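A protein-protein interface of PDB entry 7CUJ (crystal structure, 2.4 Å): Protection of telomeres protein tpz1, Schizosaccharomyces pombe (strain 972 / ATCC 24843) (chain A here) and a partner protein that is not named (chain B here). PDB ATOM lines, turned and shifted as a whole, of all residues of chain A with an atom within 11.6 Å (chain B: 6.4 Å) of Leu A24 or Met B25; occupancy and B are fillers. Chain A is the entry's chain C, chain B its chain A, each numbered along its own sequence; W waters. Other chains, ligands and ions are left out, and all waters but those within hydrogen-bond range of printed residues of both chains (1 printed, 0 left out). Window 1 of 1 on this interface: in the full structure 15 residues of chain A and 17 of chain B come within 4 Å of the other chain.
OG1 of Thr A23 sits at hydrogen-bond distance from NH2 of Arg B28, 3.0 Å away.
The guanidinium group (NH1) of Arg B28 lies within salt-bridge range of the side-chain carboxylate (OE1) of Glu A30, 3.7 Å away.
NZ of Lys B24 lies within hydrogen-bond range of ND1 of His A31, 3.4 Å away.
Among the printed residues, merely in contact across the chains: Leu A20 with Leu B29 (3.6 Å), Leu A20 with Ser B59 (3.6 Å), Glu A21 with Tyr B70 (3.9 Å), Leu A24 with Met B25 (3.6 Å), Leu A24 with Tyr B70 (3.8 Å), Gln A25 with Tyr B70 (3.3 Å), Leu A27 with Lys B24 (3.9 Å), Leu A27 with Arg B28 (3.5 Å), Tyr A28 with Leu B21 (3.9 Å), Tyr A28 with Met B25 (3.8 Å), Tyr A28 with Pro B67 (3.5 Å), Tyr A28 with Ser B68 (3.3 Å), Tyr A28 with Tyr B70 (3.6 Å), Tyr A28 with Asp B71 (3.3 Å) and His A31 with Leu B21 (3.7 Å).
Of chain A, only Leu A24 and Tyr A28 come within 4 Å of Met B25.
Leu B21 touches two residues of chain A.
No residue of chain A comes within 4 Å of Met B26.
Arg B28 touches just these residues of chain A: Thr A23 (3.0 Å), Leu A27 (3.5 Å) and Glu A30 (3.7 Å).
Leu B29 touches one residue of chain A.
Of the printed residues of chain A, Tyr B70 touches Glu A21, Leu A24, Gln A25 and Tyr A28.
Printed residues of chain B within 4 Å of Gln A25: Tyr B70.
Printed residues of chain B within 4 Å of Glu A30: Arg B28.
The nearest residue of chain A that does not touch Met B25 is Leu A27 (4.2 Å).
The nearest printed residue of chain B that does not touch Gln A25 is Asp B71 (5.0 Å).
Of the 18 printed residues of chain A, 9 touch a printed residue of chain B.
Hydrophobic or aromatic side chains of chain A that line the printed part of chain B: Leu A20, Leu A24, Leu A27, Tyr A28 and His A31.
Hydrophobic or aromatic side chains of chain B within 4 Å of the printed part of chain A: Leu B21, Met B25, Leu B29 and Tyr B70.
Among the printed residues, Asp or Glu carboxylates within 4 Å of a Lys or Arg side-chain nitrogen of the other chain: Glu A30 with Arg B28.
Water W1 lies within hydrogen-bond range of the side-chain hydroxyl of Ser B59, the side-chain hydroxyl of Tyr B70 and the side-chain carboxylate of Glu A21.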
ATOM      1  N   ASP A  15       5.671  34.338 -27.778  1.00  0.00           N
ATOM      2  CA  ASP A  15       4.434  34.943 -28.239  1.00  0.00           C
ATOM      3  C   ASP A  15       3.287  34.372 -27.409  1.00  0.00           C
ATOM      4  O   ASP A  15       2.860  33.242 -27.635  1.00  0.00           O
ATOM      5  CB  ASP A  15       4.242  34.700 -29.740  1.00  0.00           C
ATOM      6  CG  ASP A  15       3.162  35.554 -30.385  1.00  0.00           C
ATOM      7  OD1 ASP A  15       2.135  35.814 -29.726  1.00  0.00           O
ATOM      8  OD2 ASP A  15       3.362  35.955 -31.545  1.00  0.00           O
ATOM      9  N   PHE A  16       2.790  35.166 -26.455  1.00  0.00           N
ATOM     10  CA  PHE A  16       1.843  34.666 -25.470  1.00  0.00           C
ATOM     11  C   PHE A  16       0.561  34.183 -26.147  1.00  0.00           C
ATOM     12  O   PHE A  16       0.152  33.041 -25.948  1.00  0.00           O
ATOM     13  CB  PHE A  16       1.550  35.707 -24.388  1.00  0.00           C
ATOM     14  CG  PHE A  16       0.627  35.212 -23.303  1.00  0.00           C
ATOM     15  CD1 PHE A  16       1.092  34.355 -22.313  1.00  0.00           C
ATOM     16  CD2 PHE A  16      -0.711  35.583 -23.279  1.00  0.00           C
ATOM     17  CE1 PHE A  16       0.245  33.896 -21.315  1.00  0.00           C
ATOM     18  CE2 PHE A  16      -1.557  35.121 -22.281  1.00  0.00           C
ATOM     19  CZ  PHE A  16      -1.077  34.280 -21.300  1.00  0.00           C
ATOM     20  N   MET A  17      -0.054  35.061 -26.948  1.00  0.00           N
ATOM     21  CA  MET A  17      -1.344  34.791 -27.567  1.00  0.00           C
ATOM     22  C   MET A  17      -1.261  33.599 -28.522  1.00  0.00           C
ATOM     23  O   MET A  17      -2.196  32.806 -28.585  1.00  0.00           O
ATOM     24  CB  MET A  17      -1.875  36.022 -28.310  1.00  0.00           C
ATOM     25  CG  MET A  17      -2.412  37.104 -27.386  1.00  0.00           C
ATOM     26  SD  MET A  17      -3.152  38.509 -28.273  1.00  0.00           S
ATOM     27  CE  MET A  17      -4.598  37.740 -29.004  1.00  0.00           C
ATOM     28  N   LYS A  18      -0.141  33.472 -29.246  1.00  0.00           N
ATOM     29  CA  LYS A  18       0.029  32.425 -30.244  1.00  0.00           C
ATOM     30  C   LYS A  18       0.295  31.077 -29.576  1.00  0.00           C
ATOM     31  O   LYS A  18      -0.230  30.058 -30.019  1.00  0.00           O
ATOM     32  CB  LYS A  18       1.149  32.775 -31.229  1.00  0.00           C
ATOM     33  CG  LYS A  18       1.195  31.917 -32.485  1.00  0.00           C
ATOM     34  CD  LYS A  18       2.168  32.434 -33.519  1.00  0.00           C
ATOM     35  CE  LYS A  18       1.933  31.860 -34.901  1.00  0.00           C
ATOM     36  NZ  LYS A  18       2.884  32.420 -35.891  1.00  0.00           N
ATOM     37  N   GLY A  19       1.118  31.082 -28.519  1.00  0.00           N
ATOM     38  CA  GLY A  19       1.459  29.870 -27.790  1.00  0.00           C
ATOM     39  C   GLY A  19       0.242  29.223 -27.128  1.00  0.00           C
ATOM     40  O   GLY A  19       0.235  28.015 -26.893  1.00  0.00           O
ATOM     41  N   LEU A  20      -0.779  30.037 -26.829  1.00  0.00           N
ATOM     42  CA  LEU A  20      -2.018  29.561 -26.234  1.00  0.00           C
ATOM     43  C   LEU A  20      -2.778  28.702 -27.243  1.00  0.00           C
ATOM     44  O   LEU A  20      -3.168  27.576 -26.934  1.00  0.00           O
ATOM     45  CB  LEU A  20      -2.856  30.759 -25.772  1.00  0.00           C
ATOM     46  CG  LEU A  20      -4.276  30.432 -25.306  1.00  0.00           C
ATOM     47  CD1 LEU A  20      -4.259  29.469 -24.125  1.00  0.00           C
ATOM     48  CD2 LEU A  20      -5.036  31.702 -24.949  1.00  0.00           C
ATOM     49  N   GLU A  21      -2.980  29.249 -28.449  1.00  0.00           N
ATOM     50  CA  GLU A  21      -3.628  28.523 -29.529  1.00  0.00           C
ATOM     51  C   GLU A  21      -2.865  27.223 -29.774  1.00  0.00           C
ATOM     52  O   GLU A  21      -3.463  26.155 -29.806  1.00  0.00           O
ATOM     53  CB  GLU A  21      -3.730  29.380 -30.794  1.00  0.00           C
ATOM     54  CG  GLU A  21      -4.563  30.646 -30.628  1.00  0.00           C
ATOM     55  CD  GLU A  21      -6.029  30.462 -30.251  1.00  0.00           C
ATOM     56  OE1 GLU A  21      -6.823  30.033 -31.128  1.00  0.00           O
ATOM     57  OE2 GLU A  21      -6.378  30.756 -29.080  1.00  0.00           O
ATOM     58  N   THR A  22      -1.537  27.327 -29.886  1.00  0.00           N
ATOM     59  CA  THR A  22      -0.674  26.183 -30.136  1.00  0.00           C
ATOM     60  C   THR A  22      -0.900  25.085 -29.098  1.00  0.00           C
ATOM     61  O   THR A  22      -1.152  23.944 -29.469  1.00  0.00           O
ATOM     62  CB  THR A  22       0.799  26.596 -30.263  1.00  0.00           C
ATOM     63  OG1 THR A  22       0.900  27.520 -31.348  1.00  0.00           O
ATOM     64  CG2 THR A  22       1.727  25.426 -30.515  1.00  0.00           C
ATOM     65  N   THR A  23      -0.819  25.434 -27.806  1.00  0.00           N
ATOM     66  CA  THR A  23      -0.830  24.444 -26.736  1.00  0.00           C
ATOM     67  C   THR A  23      -2.203  23.783 -26.602  1.00  0.00           C
ATOM     68  O   THR A  23      -2.289  22.605 -26.262  1.00  0.00           O
ATOM     69  CB  THR A  23      -0.289  25.012 -25.415  1.00  0.00           C
ATOM     70  OG1 THR A  23      -0.111  23.925 -24.506  1.00  0.00           O
ATOM     71  CG2 THR A  23      -1.199  26.035 -24.771  1.00  0.00           C
ATOM     72  N   LEU A  24      -3.270  24.551 -26.852  1.00  0.00           N
ATOM     73  CA  LEU A  24      -4.635  24.045 -26.778  1.00  0.00           C
ATOM     74  C   LEU A  24      -4.917  23.096 -27.944  1.00  0.00           C
ATOM     75  O   LEU A  24      -5.563  22.068 -27.756  1.00  0.00           O
ATOM     76  CB  LEU A  24      -5.607  25.231 -26.760  1.00  0.00           C
ATOM     77  CG  LEU A  24      -6.374  25.492 -25.459  1.00  0.00           C
ATOM     78  CD1 LEU A  24      -5.602  25.055 -24.220  1.00  0.00           C
ATOM     79  CD2 LEU A  24      -6.784  26.951 -25.353  1.00  0.00           C
ATOM     80  N   GLN A  25      -4.417  23.446 -29.139  1.00  0.00           N
ATOM     81  CA  GLN A  25      -4.575  22.640 -30.345  1.00  0.00           C
ATOM     82  C   GLN A  25      -3.716  21.382 -30.250  1.00  0.00           C
ATOM     83  O   GLN A  25      -4.108  20.318 -30.729  1.00  0.00           O
ATOM     84  CB  GLN A  25      -4.155  23.424 -31.591  1.00  0.00           C
ATOM     85  CG  GLN A  25      -5.117  24.535 -31.988  1.00  0.00           C
ATOM     86  CD  GLN A  25      -4.645  25.317 -33.189  1.00  0.00           C
ATOM     87  OE1 GLN A  25      -3.451  25.519 -33.403  1.00  0.00           O
ATOM     88  NE2 GLN A  25      -5.593  25.772 -33.991  1.00  0.00           N
ATOM     89  N   GLU A  26      -2.536  21.526 -29.638  1.00  0.00           N
ATOM     90  CA  GLU A  26      -1.590  20.438 -29.456  1.00  0.00           C
ATOM     91  C   GLU A  26      -2.189  19.400 -28.510  1.00  0.00           C
ATOM     92  O   GLU A  26      -1.933  18.209 -28.656  1.00  0.00           O
ATOM     93  CB  GLU A  26      -0.277  20.996 -28.904  1.00  0.00           C
ATOM     94  CG  GLU A  26       0.863  19.997 -28.880  1.00  0.00           C
ATOM     95  CD  GLU A  26       2.233  20.650 -28.946  1.00  0.00           C
ATOM     96  OE1 GLU A  26       2.949  20.625 -27.922  1.00  0.00           O
ATOM     97  OE2 GLU A  26       2.579  21.182 -30.025  1.00  0.00           O
ATOM     98  N   LEU A  27      -2.992  19.870 -27.548  1.00  0.00           N
ATOM     99  CA  LEU A  27      -3.640  18.984 -26.596  1.00  0.00           C
ATOM    100  C   LEU A  27      -4.759  18.220 -27.302  1.00  0.00           C
ATOM    101  O   LEU A  27      -4.981  17.044 -27.019  1.00  0.00           O
ATOM    102  CB  LEU A  27      -4.172  19.791 -25.406  1.00  0.00           C
ATOM    103  CG  LEU A  27      -4.324  19.017 -24.095  1.00  0.00           C
ATOM    104  CD1 LEU A  27      -4.477  19.963 -22.920  1.00  0.00           C
ATOM    105  CD2 LEU A  27      -5.507  18.060 -24.143  1.00  0.00           C
ATOM    106  N   TYR A  28      -5.449  18.895 -28.228  1.00  0.00           N
ATOM    107  CA  TYR A  28      -6.533  18.272 -28.969  1.00  0.00           C
ATOM    108  C   TYR A  28      -6.025  17.039 -29.715  1.00  0.00           C
ATOM    109  O   TYR A  28      -6.673  15.995 -29.686  1.00  0.00           O
ATOM    110  CB  TYR A  28      -7.220  19.269 -29.906  1.00  0.00           C
ATOM    111  CG  TYR A  28      -8.559  18.793 -30.408  1.00  0.00           C
ATOM    112  CD1 TYR A  28      -9.715  19.032 -29.681  1.00  0.00           C
ATOM    113  CD2 TYR A  28      -8.671  18.077 -31.590  1.00  0.00           C
ATOM    114  CE1 TYR A  28     -10.949  18.586 -30.122  1.00  0.00           C
ATOM    115  CE2 TYR A  28      -9.897  17.618 -32.041  1.00  0.00           C
ATOM    116  CZ  TYR A  28     -11.042  17.879 -31.308  1.00  0.00           C
ATOM    117  OH  TYR A  28     -12.255  17.438 -31.750  1.00  0.00           O
ATOM    118  N   VAL A  29      -4.857  17.164 -30.361  1.00  0.00           N
ATOM    119  CA  VAL A  29      -4.305  16.081 -31.163  1.00  0.00           C
ATOM    120  C   VAL A  29      -3.745  14.974 -30.268  1.00  0.00           C
ATOM    121  O   VAL A  29      -3.686  13.819 -30.683  1.00  0.00           O
ATOM    122  CB  VAL A  29      -3.287  16.559 -32.222  1.00  0.00           C
ATOM    123  CG1 VAL A  29      -3.920  17.490 -33.245  1.00  0.00           C
ATOM    124  CG2 VAL A  29      -2.047  17.193 -31.611  1.00  0.00           C
ATOM    125  N   GLU A  30      -3.345  15.326 -29.040  1.00  0.00           N
ATOM    126  CA  GLU A  30      -2.890  14.340 -28.071  1.00  0.00           C
ATOM    127  C   GLU A  30      -4.049  13.415 -27.698  1.00  0.00           C
ATOM    128  O   GLU A  30      -3.857  12.214 -27.522  1.00  0.00           O
ATOM    129  CB  GLU A  30      -2.300  15.020 -26.831  1.00  0.00           C
ATOM    130  CG  GLU A  30      -0.904  15.582 -27.042  1.00  0.00           C
ATOM    131  CD  GLU A  30      -0.395  16.509 -25.948  1.00  0.00           C
ATOM    132  OE1 GLU A  30      -0.802  16.333 -24.779  1.00  0.00           O
ATOM    133  OE2 GLU A  30       0.410  17.411 -26.267  1.00  0.00           O
ATOM    134  N   HIS A  31      -5.252  13.990 -27.596  1.00  0.00           N
ATOM    135  CA  HIS A  31      -6.450  13.245 -27.243  1.00  0.00           C
ATOM    136  C   HIS A  31      -6.845  12.285 -28.365  1.00  0.00           C
ATOM    137  O   HIS A  31      -7.318  11.183 -28.094  1.00  0.00           O
ATOM    138  CB  HIS A  31      -7.592  14.204 -26.883  1.00  0.00           C
ATOM    139  CG  HIS A  31      -8.803  13.514 -26.353  1.00  0.00           C
ATOM    140  ND1 HIS A  31      -8.871  13.038 -25.057  1.00  0.00           N
ATOM    141  CD2 HIS A  31      -9.989  13.222 -26.930  1.00  0.00           C
ATOM    142  CE1 HIS A  31     -10.048  12.480 -24.858  1.00  0.00           C
ATOM    143  NE2 HIS A  31     -10.753  12.579 -25.993  1.00  0.00           N
ATOM    144  N   GLN A  32      -6.659  12.724 -29.618  1.00  0.00           N
ATOM    145  CA  GLN A  32      -6.987  11.936 -30.796  1.00  0.00           C
ATOM    146  C   GLN A  32      -6.154  10.658 -30.813  1.00  0.00           C
ATOM    147  O   GLN A  32      -6.680   9.580 -31.084  1.00  0.00           O
ATOM    148  CB  GLN A  32      -6.721  12.735 -32.072  1.00  0.00           C
ATOM    149  CG  GLN A  32      -7.847  13.682 -32.463  1.00  0.00           C
ATOM    150  CD  GLN A  32      -7.644  14.257 -33.844  1.00  0.00           C
ATOM    151  OE1 GLN A  32      -6.560  14.727 -34.193  1.00  0.00           O
ATOM    152  NE2 GLN A  32      -8.697  14.230 -34.646  1.00  0.00           N
ATOM    153  N   ALA B  20     -13.574  14.527 -20.231  1.00  0.00           N
ATOM    154  CA  ALA B  20     -12.189  14.439 -19.792  1.00  0.00           C
ATOM    155  C   ALA B  20     -11.326  15.428 -20.574  1.00  0.00           C
ATOM    156  O   ALA B  20     -10.443  16.063 -20.000  1.00  0.00           O
ATOM    157  CB  ALA B  20     -11.683  13.022 -19.925  1.00  0.00           C
ATOM    158  N   LEU B  21     -11.615  15.563 -21.876  1.00  0.00           N
ATOM    159  CA  LEU B  21     -10.909  16.449 -22.792  1.00  0.00           C
ATOM    160  C   LEU B  21     -11.062  17.897 -22.330  1.00  0.00           C
ATOM    161  O   LEU B  21     -10.082  18.634 -22.265  1.00  0.00           O
ATOM    162  CB  LEU B  21     -11.504  16.279 -24.196  1.00  0.00           C
ATOM    163  CG  LEU B  21     -10.606  16.601 -25.395  1.00  0.00           C
ATOM    164  CD1 LEU B  21     -11.450  16.975 -26.604  1.00  0.00           C
ATOM    165  CD2 LEU B  21      -9.596  17.699 -25.101  1.00  0.00           C
ATOM    166  N   GLN B  22     -12.304  18.295 -22.034  1.00  0.00           N
ATOM    167  CA  GLN B  22     -12.620  19.659 -21.645  1.00  0.00           C
ATOM    168  C   GLN B  22     -11.880  20.023 -20.360  1.00  0.00           C
ATOM    169  O   GLN B  22     -11.395  21.142 -20.223  1.00  0.00           O
ATOM    170  CB  GLN B  22     -14.132  19.826 -21.469  1.00  0.00           C
ATOM    171  CG  GLN B  22     -14.880  20.114 -22.761  1.00  0.00           C
ATOM    172  CD  GLN B  22     -16.379  20.139 -22.578  1.00  0.00           C
ATOM    173  OE1 GLN B  22     -16.963  19.268 -21.941  1.00  0.00           O
ATOM    174  NE2 GLN B  22     -17.023  21.143 -23.148  1.00  0.00           N
ATOM    175  N   ARG B  23     -11.800  19.066 -19.426  1.00  0.00           N
ATOM    176  CA  ARG B  23     -11.152  19.277 -18.140  1.00  0.00           C
ATOM    177  C   ARG B  23      -9.647  19.440 -18.335  1.00  0.00           C
ATOM    178  O   ARG B  23      -9.037  20.318 -17.726  1.00  0.00           O
ATOM    179  CB  ARG B  23     -11.472  18.132 -17.175  1.00  0.00           C
ATOM    180  CG  ARG B  23     -12.911  18.138 -16.684  1.00  0.00           C
ATOM    181  CD  ARG B  23     -13.465  16.735 -16.560  1.00  0.00           C
ATOM    182  NE  ARG B  23     -13.744  16.371 -15.181  1.00  0.00           N
ATOM    183  CZ  ARG B  23     -14.948  16.063 -14.707  1.00  0.00           C
ATOM    184  NH1 ARG B  23     -16.003  16.059 -15.507  1.00  0.00           N
ATOM    185  NH2 ARG B  23     -15.091  15.748 -13.432  1.00  0.00           N
ATOM    186  N   LYS B  24      -9.065  18.582 -19.182  1.00  0.00           N
ATOM    187  CA  LYS B  24      -7.657  18.671 -19.522  1.00  0.00           C
ATOM    188  C   LYS B  24      -7.363  20.063 -20.068  1.00  0.00           C
ATOM    189  O   LYS B  24      -6.395  20.700 -19.659  1.00  0.00           O
ATOM    190  CB  LYS B  24      -7.290  17.642 -20.592  1.00  0.00           C
ATOM    191  CG  LYS B  24      -7.042  16.228 -20.097  1.00  0.00           C
ATOM    192  CD  LYS B  24      -6.514  15.359 -21.211  1.00  0.00           C
ATOM    193  CE  LYS B  24      -6.781  13.887 -21.000  1.00  0.00           C
ATOM    194  NZ  LYS B  24      -6.817  13.159 -22.291  1.00  0.00           N
ATOM    195  N   MET B  25      -8.225  20.522 -20.982  1.00  0.00           N
ATOM    196  CA  MET B  25      -8.048  21.796 -21.656  1.00  0.00           C
ATOM    197  C   MET B  25      -8.135  22.944 -20.654  1.00  0.00           C
ATOM    198  O   MET B  25      -7.372  23.902 -20.745  1.00  0.00           O
ATOM    199  CB  MET B  25      -9.100  21.987 -22.751  1.00  0.00           C
ATOM    200  CG  MET B  25      -8.762  21.257 -24.032  1.00  0.00           C
ATOM    201  SD  MET B  25      -9.955  21.662 -25.329  1.00  0.00           S
ATOM    202  CE  MET B  25      -8.967  21.341 -26.788  1.00  0.00           C
ATOM    203  N   MET B  26      -9.065  22.827 -19.700  1.00  0.00           N
ATOM    204  CA  MET B  26      -9.236  23.817 -18.651  1.00  0.00           C
ATOM    205  C   MET B  26      -7.996  23.844 -17.761  1.00  0.00           C
ATOM    206  O   MET B  26      -7.557  24.912 -17.348  1.00  0.00           O
ATOM    207  CB  MET B  26     -10.478  23.518 -17.802  1.00  0.00           C
ATOM    208  CG  MET B  26     -11.783  23.916 -18.466  1.00  0.00           C
ATOM    209  SD  MET B  26     -11.794  25.621 -19.090  1.00  0.00           S
ATOM    210  CE  MET B  26     -11.548  26.533 -17.566  1.00  0.00           C
ATOM    211  N   HIS B  27      -7.441  22.657 -17.484  1.00  0.00           N
ATOM    212  CA  HIS B  27      -6.248  22.513 -16.667  1.00  0.00           C
ATOM    213  C   HIS B  27      -5.053  23.148 -17.378  1.00  0.00           C
ATOM    214  O   HIS B  27      -4.292  23.886 -16.759  1.00  0.00           O
ATOM    215  CB  HIS B  27      -6.038  21.042 -16.275  1.00  0.00           C
ATOM    216  CG  HIS B  27      -4.695  20.748 -15.693  1.00  0.00           C
ATOM    217  ND1 HIS B  27      -4.492  20.617 -14.330  1.00  0.00           N
ATOM    218  CD2 HIS B  27      -3.491  20.551 -16.275  1.00  0.00           C
ATOM    219  CE1 HIS B  27      -3.221  20.354 -14.099  1.00  0.00           C
ATOM    220  NE2 HIS B  27      -2.586  20.308 -15.277  1.00  0.00           N
ATOM    221  N   ARG B  28      -4.917  22.870 -18.681  1.00  0.00           N
ATOM    222  CA  ARG B  28      -3.838  23.399 -19.502  1.00  0.00           C
ATOM    223  C   ARG B  28      -3.935  24.922 -19.566  1.00  0.00           C
ATOM    224  O   ARG B  28      -2.918  25.613 -19.490  1.00  0.00           O
ATOM    225  CB  ARG B  28      -3.885  22.783 -20.906  1.00  0.00           C
ATOM    226  CG  ARG B  28      -2.761  23.210 -21.846  1.00  0.00           C
ATOM    227  CD  ARG B  28      -1.375  22.675 -21.510  1.00  0.00           C
ATOM    228  NE  ARG B  28      -1.276  21.217 -21.523  1.00  0.00           N
ATOM    229  CZ  ARG B  28      -0.899  20.477 -22.565  1.00  0.00           C
ATOM    230  NH1 ARG B  28      -0.850  19.160 -22.450  1.00  0.00           N
ATOM    231  NH2 ARG B  28      -0.573  21.047 -23.714  1.00  0.00           N
ATOM    232  N   LEU B  29      -5.169  25.425 -19.698  1.00  0.00           N
ATOM    233  CA  LEU B  29      -5.438  26.846 -19.865  1.00  0.00           C
ATOM    234  C   LEU B  29      -5.006  27.621 -18.621  1.00  0.00           C
ATOM    235  O   LEU B  29      -4.315  28.632 -18.733  1.00  0.00           O
ATOM    236  CB  LEU B  29      -6.931  27.038 -20.153  1.00  0.00           C
ATOM    237  CG  LEU B  29      -7.396  28.486 -20.287  1.00  0.00           C
ATOM    238  CD1 LEU B  29      -6.746  29.158 -21.490  1.00  0.00           C
ATOM    239  CD2 LEU B  29      -8.912  28.565 -20.370  1.00  0.00           C
ATOM    240  N   VAL B  30      -5.418  27.135 -17.442  1.00  0.00           N
ATOM    241  CA  VAL B  30      -5.114  27.781 -16.177  1.00  0.00           C
ATOM    242  C   VAL B  30      -3.604  27.756 -15.940  1.00  0.00           C
ATOM    243  O   VAL B  30      -3.043  28.728 -15.447  1.00  0.00           O
ATOM    244  CB  VAL B  30      -5.898  27.140 -15.015  1.00  0.00           C
ATOM    245  CG1 VAL B  30      -5.351  27.550 -13.656  1.00  0.00           C
ATOM    246  CG2 VAL B  30      -7.386  27.446 -15.107  1.00  0.00           C
ATOM    247  N   SER B  59     -11.261  31.919 -23.951  1.00  0.00           N
ATOM    248  CA  SER B  59     -10.799  30.550 -24.139  1.00  0.00           C
ATOM    249  C   SER B  59     -11.617  29.575 -23.294  1.00  0.00           C
ATOM    250  O   SER B  59     -11.901  28.468 -23.741  1.00  0.00           O
ATOM    251  CB  SER B  59      -9.337  30.430 -23.806  1.00  0.00           C
ATOM    252  OG  SER B  59      -8.572  31.358 -24.551  1.00  0.00           O
ATOM    253  N   ILE B  63     -13.930  26.458 -24.659  1.00  0.00           N
ATOM    254  CA  ILE B  63     -13.808  25.085 -24.190  1.00  0.00           C
ATOM    255  C   ILE B  63     -15.178  24.584 -23.734  1.00  0.00           C
ATOM    256  O   ILE B  63     -15.526  23.427 -23.965  1.00  0.00           O
ATOM    257  CB  ILE B  63     -12.733  24.974 -23.085  1.00  0.00           C
ATOM    258  CG1 ILE B  63     -11.329  25.232 -23.646  1.00  0.00           C
ATOM    259  CG2 ILE B  63     -12.808  23.634 -22.363  1.00  0.00           C
ATOM    260  CD1 ILE B  63     -10.315  25.691 -22.616  1.00  0.00           C
ATOM    261  N   HIS B  66     -17.440  24.033 -27.137  1.00  0.00           N
ATOM    262  CA  HIS B  66     -17.004  22.752 -27.671  1.00  0.00           C
ATOM    263  C   HIS B  66     -15.484  22.719 -27.764  1.00  0.00           C
ATOM    264  O   HIS B  66     -14.880  23.654 -28.283  1.00  0.00           O
ATOM    265  CB  HIS B  66     -17.634  22.492 -29.044  1.00  0.00           C
ATOM    266  CG  HIS B  66     -17.768  21.041 -29.359  1.00  0.00           C
ATOM    267  ND1 HIS B  66     -18.983  20.393 -29.313  1.00  0.00           N
ATOM    268  CD2 HIS B  66     -16.854  20.108 -29.702  1.00  0.00           C
ATOM    269  CE1 HIS B  66     -18.816  19.126 -29.632  1.00  0.00           C
ATOM    270  NE2 HIS B  66     -17.517  18.925 -29.871  1.00  0.00           N
ATOM    271  N   PRO B  67     -14.819  21.644 -27.282  1.00  0.00           N
ATOM    272  CA  PRO B  67     -13.361  21.542 -27.368  1.00  0.00           C
ATOM    273  C   PRO B  67     -12.815  21.544 -28.796  1.00  0.00           C
ATOM    274  O   PRO B  67     -11.665  21.921 -29.017  1.00  0.00           O
ATOM    275  CB  PRO B  67     -13.038  20.224 -26.643  1.00  0.00           C
ATOM    276  CG  PRO B  67     -14.340  19.444 -26.657  1.00  0.00           C
ATOM    277  CD  PRO B  67     -15.430  20.491 -26.597  1.00  0.00           C
ATOM    278  N   SER B  68     -13.655  21.152 -29.762  1.00  0.00           N
ATOM    279  CA  SER B  68     -13.229  21.018 -31.147  1.00  0.00           C
ATOM    280  C   SER B  68     -13.077  22.382 -31.824  1.00  0.00           C
ATOM    281  O   SER B  68     -12.692  22.446 -32.988  1.00  0.00           O
ATOM    282  CB  SER B  68     -14.133  20.094 -31.922  1.00  0.00           C
ATOM    283  OG  SER B  68     -15.400  20.695 -32.135  1.00  0.00           O
ATOM    284  N   TYR B  70     -10.723  23.945 -31.031  1.00  0.00           N
ATOM    285  CA  TYR B  70      -9.265  23.927 -31.063  1.00  0.00           C
ATOM    286  C   TYR B  70      -8.753  22.753 -31.895  1.00  0.00           C
ATOM    287  O   TYR B  70      -7.596  22.357 -31.773  1.00  0.00           O
ATOM    288  CB  TYR B  70      -8.671  24.000 -29.651  1.00  0.00           C
ATOM    289  CG  TYR B  70      -9.001  25.294 -28.955  1.00  0.00           C
ATOM    290  CD1 TYR B  70      -8.322  26.463 -29.263  1.00  0.00           C
ATOM    291  CD2 TYR B  70     -10.033  25.365 -28.035  1.00  0.00           C
ATOM    292  CE1 TYR B  70      -8.641  27.667 -28.656  1.00  0.00           C
ATOM    293  CE2 TYR B  70     -10.365  26.560 -27.418  1.00  0.00           C
ATOM    294  CZ  TYR B  70      -9.670  27.715 -27.734  1.00  0.00           C
ATOM    295  OH  TYR B  70      -9.998  28.899 -27.138  1.00  0.00           O
ATOM    296  N   ASP B  71      -9.629  22.213 -32.749  1.00  0.00           N
ATOM    297  CA  ASP B  71      -9.236  21.275 -33.787  1.00  0.00           C
ATOM    298  C   ASP B  71      -8.819  22.083 -35.011  1.00  0.00           C
ATOM    299  O   ASP B  71      -9.528  23.002 -35.413  1.00  0.00           O
ATOM    300  CB  ASP B  71     -10.386  20.321 -34.121  1.00  0.00           C
ATOM    301  CG  ASP B  71      -9.996  19.128 -34.980  1.00  0.00           C
ATOM    302  OD1 ASP B  71      -8.808  19.024 -35.347  1.00  0.00           O
ATOM    303  OD2 ASP B  71     -10.892  18.304 -35.270  1.00  0.00           O
HETATM  304  O   HOH W   1      -8.292  30.911 -27.120  1.00  0.00           O
